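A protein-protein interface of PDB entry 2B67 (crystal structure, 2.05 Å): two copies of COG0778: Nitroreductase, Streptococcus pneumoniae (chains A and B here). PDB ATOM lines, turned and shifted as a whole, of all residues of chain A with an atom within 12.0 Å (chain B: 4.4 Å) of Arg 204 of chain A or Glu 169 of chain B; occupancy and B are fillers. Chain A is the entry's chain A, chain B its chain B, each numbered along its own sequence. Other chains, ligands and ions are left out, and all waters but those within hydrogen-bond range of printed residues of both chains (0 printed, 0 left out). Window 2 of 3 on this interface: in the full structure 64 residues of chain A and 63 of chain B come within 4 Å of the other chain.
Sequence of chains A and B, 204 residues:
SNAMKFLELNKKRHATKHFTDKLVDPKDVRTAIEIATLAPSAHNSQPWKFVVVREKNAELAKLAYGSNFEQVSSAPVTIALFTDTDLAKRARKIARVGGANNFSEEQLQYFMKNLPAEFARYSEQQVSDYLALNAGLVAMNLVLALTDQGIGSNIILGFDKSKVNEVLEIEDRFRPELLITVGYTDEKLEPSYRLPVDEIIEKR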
ATOM      1  N   ASP A 198     -16.413  20.149 -29.512  1.00  0.00           N
ATOM      2  CA  ASP A 198     -15.307  19.193 -29.360  1.00  0.00           C
ATOM      3  C   ASP A 198     -15.184  18.646 -27.933  1.00  0.00           C
ATOM      4  O   ASP A 198     -14.626  17.579 -27.733  1.00  0.00           O
ATOM      5  CB  ASP A 198     -13.981  19.798 -29.855  1.00  0.00           C
ATOM      6  CG  ASP A 198     -14.058  20.262 -31.315  1.00  0.00           C
ATOM      7  OD1 ASP A 198     -13.677  21.431 -31.567  1.00  0.00           O
ATOM      8  OD2 ASP A 198     -14.530  19.489 -32.201  1.00  0.00           O
ATOM      9  N   GLU A 199     -15.726  19.366 -26.951  1.00  0.00           N
ATOM     10  CA  GLU A 199     -15.784  18.869 -25.566  1.00  0.00           C
ATOM     11  C   GLU A 199     -16.709  17.663 -25.369  1.00  0.00           C
ATOM     12  O   GLU A 199     -16.543  16.910 -24.405  1.00  0.00           O
ATOM     13  CB  GLU A 199     -16.238  19.983 -24.613  1.00  0.00           C
ATOM     14  CG  GLU A 199     -16.049  19.666 -23.142  1.00  0.00           C
ATOM     15  CD  GLU A 199     -14.564  19.479 -22.773  1.00  0.00           C
ATOM     16  OE1 GLU A 199     -14.135  18.313 -22.584  1.00  0.00           O
ATOM     17  OE2 GLU A 199     -13.830  20.494 -22.690  1.00  0.00           O
ATOM     18  N   ILE A 200     -17.703  17.507 -26.248  1.00  0.00           N
ATOM     19  CA  ILE A 200     -18.745  16.489 -26.036  1.00  0.00           C
ATOM     20  C   ILE A 200     -18.771  15.444 -27.154  1.00  0.00           C
ATOM     21  O   ILE A 200     -19.642  14.592 -27.174  1.00  0.00           O
ATOM     22  CB  ILE A 200     -20.163  17.129 -25.860  1.00  0.00           C
ATOM     23  CG1 ILE A 200     -20.546  17.922 -27.110  1.00  0.00           C
ATOM     24  CG2 ILE A 200     -20.226  18.009 -24.599  1.00  0.00           C
ATOM     25  CD1 ILE A 200     -21.898  18.496 -27.070  1.00  0.00           C
ATOM     26  N   ILE A 201     -17.815  15.522 -28.074  1.00  0.00           N
ATOM     27  CA  ILE A 201     -17.653  14.531 -29.135  1.00  0.00           C
ATOM     28  C   ILE A 201     -16.463  13.590 -28.859  1.00  0.00           C
ATOM     29  O   ILE A 201     -15.370  14.015 -28.434  1.00  0.00           O
ATOM     30  CB  ILE A 201     -17.473  15.195 -30.521  1.00  0.00           C
ATOM     31  CG1 ILE A 201     -18.764  15.861 -30.979  1.00  0.00           C
ATOM     32  CG2 ILE A 201     -17.003  14.165 -31.570  1.00  0.00           C
ATOM     33  CD1 ILE A 201     -18.674  16.592 -32.335  1.00  0.00           C
ATOM     34  N   GLU A 202     -16.688  12.301 -29.095  1.00  0.00           N
ATOM     35  CA  GLU A 202     -15.643  11.301 -28.981  1.00  0.00           C
ATOM     36  C   GLU A 202     -15.614  10.572 -30.301  1.00  0.00           C
ATOM     37  O   GLU A 202     -16.669  10.282 -30.863  1.00  0.00           O
ATOM     38  CB  GLU A 202     -16.011  10.309 -27.895  1.00  0.00           C
ATOM     39  CG  GLU A 202     -14.863   9.719 -27.162  1.00  0.00           C
ATOM     40  CD  GLU A 202     -14.426  10.558 -25.979  1.00  0.00           C
ATOM     41  OE1 GLU A 202     -14.518  11.796 -26.065  1.00  0.00           O
ATOM     42  OE2 GLU A 202     -13.986   9.967 -24.961  1.00  0.00           O
ATOM     43  N   LYS A 203     -14.413  10.259 -30.779  1.00  0.00           N
ATOM     44  CA  LYS A 203     -14.240   9.571 -32.050  1.00  0.00           C
ATOM     45  C   LYS A 203     -13.797   8.136 -31.824  1.00  0.00           C
ATOM     46  O   LYS A 203     -12.848   7.872 -31.081  1.00  0.00           O
ATOM     47  CB  LYS A 203     -13.248  10.318 -32.937  1.00  0.00           C
ATOM     48  CG  LYS A 203     -13.654  11.756 -33.265  1.00  0.00           C
ATOM     49  CD  LYS A 203     -12.824  12.304 -34.442  1.00  0.00           C
ATOM     50  CE  LYS A 203     -13.350  13.653 -34.946  1.00  0.00           C
ATOM     51  NZ  LYS A 203     -12.931  14.793 -34.058  1.00  0.00           N
ATOM     52  N   ARG A 204     -14.522   7.214 -32.452  1.00  0.00           N
ATOM     53  CA  ARG A 204     -14.271   5.787 -32.349  1.00  0.00           C
ATOM     54  C   ARG A 204     -14.460   5.079 -33.699  1.00  0.00           C
ATOM     55  O   ARG A 204     -14.366   5.623 -34.799  1.00  0.00           O
ATOM     56  CB  ARG A 204     -15.222   5.149 -31.326  1.00  0.00           C
ATOM     57  CG  ARG A 204     -14.970   5.526 -29.895  1.00  0.00           C
ATOM     58  CD  ARG A 204     -13.571   5.117 -29.425  1.00  0.00           C
ATOM     59  NE  ARG A 204     -13.402   5.430 -28.011  1.00  0.00           N
ATOM     60  CZ  ARG A 204     -12.922   6.577 -27.535  1.00  0.00           C
ATOM     61  NH1 ARG A 204     -12.564   7.570 -28.356  1.00  0.00           N
ATOM     62  NH2 ARG A 204     -12.827   6.736 -26.223  1.00  0.00           N
ATOM     63  OXT ARG A 204     -14.765   3.894 -33.704  1.00  0.00           O
ATOM     64  N   VAL B  51     -20.731   9.855 -29.389  1.00  0.00           N
ATOM     65  CA  VAL B  51     -19.630   8.995 -29.818  1.00  0.00           C
ATOM     66  C   VAL B  51     -19.780   8.642 -31.289  1.00  0.00           C
ATOM     67  O   VAL B  51     -20.653   7.831 -31.670  1.00  0.00           O
ATOM     68  CB  VAL B  51     -19.509   7.745 -28.922  1.00  0.00           C
ATOM     69  CG1 VAL B  51     -18.334   6.851 -29.362  1.00  0.00           C
ATOM     70  CG2 VAL B  51     -19.304   8.178 -27.478  1.00  0.00           C
ATOM     71  N   VAL B  52     -18.947   9.289 -32.119  1.00  0.00           N
ATOM     72  CA  VAL B  52     -19.032   9.160 -33.571  1.00  0.00           C
ATOM     73  C   VAL B  52     -18.229   7.936 -34.015  1.00  0.00           C
ATOM     74  O   VAL B  52     -16.998   7.961 -34.004  1.00  0.00           O
ATOM     75  CB  VAL B  52     -18.592  10.469 -34.283  1.00  0.00           C
ATOM     76  CG1 VAL B  52     -18.696  10.341 -35.801  1.00  0.00           C
ATOM     77  CG2 VAL B  52     -19.485  11.657 -33.803  1.00  0.00           C
ATOM     78  N   VAL B  53     -18.933   6.857 -34.345  1.00  0.00           N
ATOM     79  CA  VAL B  53     -18.297   5.588 -34.718  1.00  0.00           C
ATOM     80  C   VAL B  53     -18.025   5.471 -36.230  1.00  0.00           C
ATOM     81  O   VAL B  53     -18.956   5.411 -37.048  1.00  0.00           O
ATOM     82  CB  VAL B  53     -19.091   4.366 -34.181  1.00  0.00           C
ATOM     83  CG1 VAL B  53     -18.319   3.023 -34.451  1.00  0.00           C
ATOM     84  CG2 VAL B  53     -19.373   4.535 -32.684  1.00  0.00           C
ATOM     85  N   ARG B  54     -16.736   5.441 -36.580  1.00  0.00           N
ATOM     86  CA  ARG B  54     -16.287   5.294 -37.966  1.00  0.00           C
ATOM     87  C   ARG B  54     -15.361   4.073 -38.137  1.00  0.00           C
ATOM     88  O   ARG B  54     -15.293   3.504 -39.226  1.00  0.00           O
ATOM     89  CB  ARG B  54     -15.593   6.566 -38.487  1.00  0.00           C
ATOM     90  CG  ARG B  54     -16.281   7.880 -38.145  1.00  0.00           C
ATOM     91  CD  ARG B  54     -15.764   9.045 -38.984  1.00  0.00           C
ATOM     92  NE  ARG B  54     -16.266   8.911 -40.342  1.00  0.00           N
ATOM     93  CZ  ARG B  54     -17.159   9.700 -40.926  1.00  0.00           C
ATOM     94  NH1 ARG B  54     -17.677  10.751 -40.297  1.00  0.00           N
ATOM     95  NH2 ARG B  54     -17.529   9.425 -42.167  1.00  0.00           N
ATOM     96  N   GLU B  55     -14.680   3.667 -37.063  1.00  0.00           N
ATOM     97  CA  GLU B  55     -13.730   2.548 -37.122  1.00  0.00           C
ATOM     98  C   GLU B  55     -14.200   1.274 -36.425  1.00  0.00           C
ATOM     99  O   GLU B  55     -13.774   0.188 -36.791  1.00  0.00           O
ATOM    100  CB  GLU B  55     -12.351   2.967 -36.574  1.00  0.00           C
ATOM    101  CG  GLU B  55     -11.719   4.155 -37.324  1.00  0.00           C
ATOM    102  CD  GLU B  55     -10.308   4.542 -36.819  1.00  0.00           C
ATOM    103  OE1 GLU B  55      -9.949   4.218 -35.652  1.00  0.00           O
ATOM    104  OE2 GLU B  55      -9.564   5.193 -37.608  1.00  0.00           O
ATOM    105  N   LYS B  56     -15.066   1.404 -35.420  1.00  0.00           N
ATOM    106  CA  LYS B  56     -15.530   0.251 -34.640  1.00  0.00           C
ATOM    107  C   LYS B  56     -16.930  -0.275 -35.020  1.00  0.00           C
ATOM    108  O   LYS B  56     -17.539  -1.038 -34.257  1.00  0.00           O
ATOM    109  CB  LYS B  56     -15.482   0.582 -33.155  1.00  0.00           C
ATOM    110  CG  LYS B  56     -14.110   0.387 -32.497  1.00  0.00           C
ATOM    111  CD  LYS B  56     -13.767   1.569 -31.609  1.00  0.00           C
ATOM    112  CE  LYS B  56     -13.249   1.148 -30.225  1.00  0.00           C
ATOM    113  NZ  LYS B  56     -11.986   0.326 -30.243  1.00  0.00           N
ATOM    114  N   ASN B 165     -20.141   0.172 -23.568  1.00  0.00           N
ATOM    115  CA  ASN B 165     -18.994   0.859 -22.981  1.00  0.00           C
ATOM    116  C   ASN B 165     -17.662   0.146 -23.286  1.00  0.00           C
ATOM    117  O   ASN B 165     -16.682   0.807 -23.672  1.00  0.00           O
ATOM    118  CB  ASN B 165     -19.142   1.048 -21.462  1.00  0.00           C
ATOM    119  CG  ASN B 165     -20.104   2.179 -21.088  1.00  0.00           C
ATOM    120  OD1 ASN B 165     -19.687   3.317 -20.848  1.00  0.00           O
ATOM    121  ND2 ASN B 165     -21.378   1.852 -20.992  1.00  0.00           N
ATOM    122  N   GLU B 166     -17.646  -1.183 -23.089  1.00  0.00           N
ATOM    123  CA  GLU B 166     -16.470  -2.042 -23.366  1.00  0.00           C
ATOM    124  C   GLU B 166     -16.072  -1.957 -24.827  1.00  0.00           C
ATOM    125  O   GLU B 166     -14.946  -1.625 -25.140  1.00  0.00           O
ATOM    126  CB  GLU B 166     -16.754  -3.506 -22.993  1.00  0.00           C
ATOM    127  CG  GLU B 166     -15.583  -4.507 -23.285  1.00  0.00           C
ATOM    128  CD  GLU B 166     -16.004  -5.990 -23.136  1.00  0.00           C
ATOM    129  OE1 GLU B 166     -15.490  -6.678 -22.198  1.00  0.00           O
ATOM    130  OE2 GLU B 166     -16.850  -6.471 -23.953  1.00  0.00           O
ATOM    131  N   VAL B 167     -17.026  -2.202 -25.719  1.00  0.00           N
ATOM    132  CA  VAL B 167     -16.789  -2.178 -27.161  1.00  0.00           C
ATOM    133  C   VAL B 167     -16.285  -0.837 -27.715  1.00  0.00           C
ATOM    134  O   VAL B 167     -15.389  -0.796 -28.571  1.00  0.00           O
ATOM    135  CB  VAL B 167     -18.070  -2.581 -27.907  1.00  0.00           C
ATOM    136  CG1 VAL B 167     -17.935  -2.351 -29.394  1.00  0.00           C
ATOM    137  CG2 VAL B 167     -18.412  -4.036 -27.602  1.00  0.00           C
ATOM    138  N   LEU B 168     -16.886   0.261 -27.255  1.00  0.00           N
ATOM    139  CA  LEU B 168     -16.536   1.589 -27.765  1.00  0.00           C
ATOM    140  C   LEU B 168     -15.483   2.272 -26.913  1.00  0.00           C
ATOM    141  O   LEU B 168     -15.102   3.401 -27.206  1.00  0.00           O
ATOM    142  CB  LEU B 168     -17.778   2.498 -27.873  1.00  0.00           C
ATOM    143  CG  LEU B 168     -18.856   2.131 -28.886  1.00  0.00           C
ATOM    144  CD1 LEU B 168     -19.818   3.306 -29.013  1.00  0.00           C
ATOM    145  CD2 LEU B 168     -18.254   1.775 -30.239  1.00  0.00           C
ATOM    146  N   GLU B 169     -15.037   1.598 -25.857  1.00  0.00           N
ATOM    147  CA  GLU B 169     -13.989   2.114 -24.953  1.00  0.00           C
ATOM    148  C   GLU B 169     -14.370   3.474 -24.366  1.00  0.00           C
ATOM    149  O   GLU B 169     -13.656   4.475 -24.546  1.00  0.00           O
ATOM    150  CB  GLU B 169     -12.627   2.178 -25.652  1.00  0.00           C
ATOM    151  CG  GLU B 169     -12.120   0.825 -26.105  1.00  0.00           C
ATOM    152  CD  GLU B 169     -10.672   0.871 -26.571  1.00  0.00           C
ATOM    153  OE1 GLU B 169     -10.449   0.656 -27.790  1.00  0.00           O
ATOM    154  OE2 GLU B 169      -9.767   1.128 -25.723  1.00  0.00           O
ATOM    155  N   ILE B 170     -15.524   3.481 -23.682  1.00  0.00           N
ATOM    156  CA  ILE B 170     -16.112   4.685 -23.097  1.00  0.00           C
ATOM    157  C   ILE B 170     -16.265   4.441 -21.592  1.00  0.00           C
ATOM    158  O   ILE B 170     -16.775   3.410 -21.187  1.00  0.00           O
ATOM    159  CB  ILE B 170     -17.495   5.033 -23.766  1.00  0.00           C
ATOM    160  CG1 ILE B 170     -17.356   5.293 -25.284  1.00  0.00           C
ATOM    161  CG2 ILE B 170     -18.186   6.206 -23.048  1.00  0.00           C
ATOM    162  CD1 ILE B 170     -16.619   6.587 -25.657  1.00  0.00           C
ATOM    163  N   GLU B 171     -15.831   5.390 -20.769  1.00  0.00           N
ATOM    164  CA  GLU B 171     -15.893   5.240 -19.318  1.00  0.00           C
ATOM    165  C   GLU B 171     -17.322   4.979 -18.856  1.00  0.00           C
ATOM    166  O   GLU B 171     -18.272   5.605 -19.351  1.00  0.00           O
ATOM    167  CB  GLU B 171     -15.331   6.476 -18.596  1.00  0.00           C
ATOM    168  CG  GLU B 171     -13.905   6.901 -19.013  1.00  0.00           C
ATOM    169  CD  GLU B 171     -12.828   5.882 -18.657  1.00  0.00           C
ATOM    170  OE1 GLU B 171     -12.349   5.893 -17.495  1.00  0.00           O
ATOM    171  OE2 GLU B 171     -12.445   5.082 -19.553  1.00  0.00           O
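No position is printed for both chains.
Of the printed residues of chain B, Lys 203 of chain A touches Val 52 (3.7 Å).
Of chain B, only Val 51 (3.7 Å), Val 52 (3.0 Å), Val 53 (3.7 Å), Arg 54 (3.0 Å), Glu 55 (3.0 Å), Lys 56 (3.0 Å), Leu 168 (2.8 Å), Glu 169 (2.9 Å) and Ile 170 (3.8 Å) come within 4 Å of Arg 204 of chain A.
Of chain A, only Glu 202 and Arg 204 come within 4 Å of Val 51 of chain B.
Val 53 of chain B touches just one residue of chain A: Arg 204 (3.7 Å).
Of the printed residues of chain A, Arg 54 of chain B touches Arg 204 (3.0 Å).
Of the printed residues of chain A, Glu 55 of chain B touches Arg 204.
Of chain A, only Arg 204 comes within 4 Å of Lys 56 of chain B.
No residue of chain A comes within 4 Å of Asn 165 of chain B.
Val 167 of chain B touches none of the printed residues of chain A.
Leu 168 of chain B touches just one residue of chain A: Arg 204.
Of the printed residues of chain A, Glu 169 of chain B touches Arg 204.
Of chain A, only Glu 202 (3.9 Å) and Arg 204 (3.8 Å) come within 4 Å of Ile 170 of chain B.
No residue of chain A comes within 4 Å of Glu 171 of chain B.
The nearest printed residue of chain B that does not touch Arg 204 of chain A is Val 167 of chain B (6.2 Å).
The backbone carbonyl oxygen (O) of Glu 202 of chain A sits at hydrogen-bond distance from the backbone NH (N) of Val 52 of chain B (2.8 Å).
The backbone carbonyl oxygen of Val 52 of chain B sits at hydrogen-bond distance from the backbone NH of Arg 204 of chain A.
O of Arg 204 of chain A lies within hydrogen-bond range of N of Arg 54 of chain B (3.0 Å).
O of Arg 204 of chain A is in hydrogen-bond range of N of Glu 55 of chain B, 3.0 Å away.
OXT of Arg 204 of chain A lies within hydrogen-bond range of N of Lys 56 of chain B (3.0 Å).
The guanidinium group (NE) of Arg 204 of chain A is in hydrogen-bond range of the backbone carbonyl oxygen (O) of Leu 168 of chain B, 2.8 Å away.
The guanidinium group (NH2) of Arg 204 of chain A lies within hydrogen-bond range of the backbone carbonyl oxygen (O) of Glu 169 of chain B (2.9 Å).
Of the 7 printed residues of chain A, 3 touch a printed residue of chain B.
Among the printed residues, 13 pairs touch across the chains.
Among the printed residues, no Asp or Glu carboxylate lies within 4 Å of a Lys or Arg side-chain nitrogen of the other chain.
The side-chain carboxylate (OE2) of Glu 202 of chain A is in salt-bridge range of the guanidinium group (NH2) of Arg 204 of chain A.
NZ of Lys 56 of chain B lies within salt-bridge range of OE1 of Glu 169 of chain B (2.9 Å).
The backbone NH (N) of Ile 170 of chain B lies within hydrogen-bond range of the backbone carbonyl oxygen (O) of Asn 165 of chain B (2.9 Å).
Among the printed residues, merely in contact across the chains: Glu 202 of chain A with Val 51 of chain B, Glu 202 of chain A with Ile 170 of chain B, Lys 203 of chain A with Val 52 of chain B, Arg 204 of chain A with Val 51 of chain B, Arg 204 of chain A with Val 53 of chain B and Arg 204 of chain A with Ile 170 of chain B.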
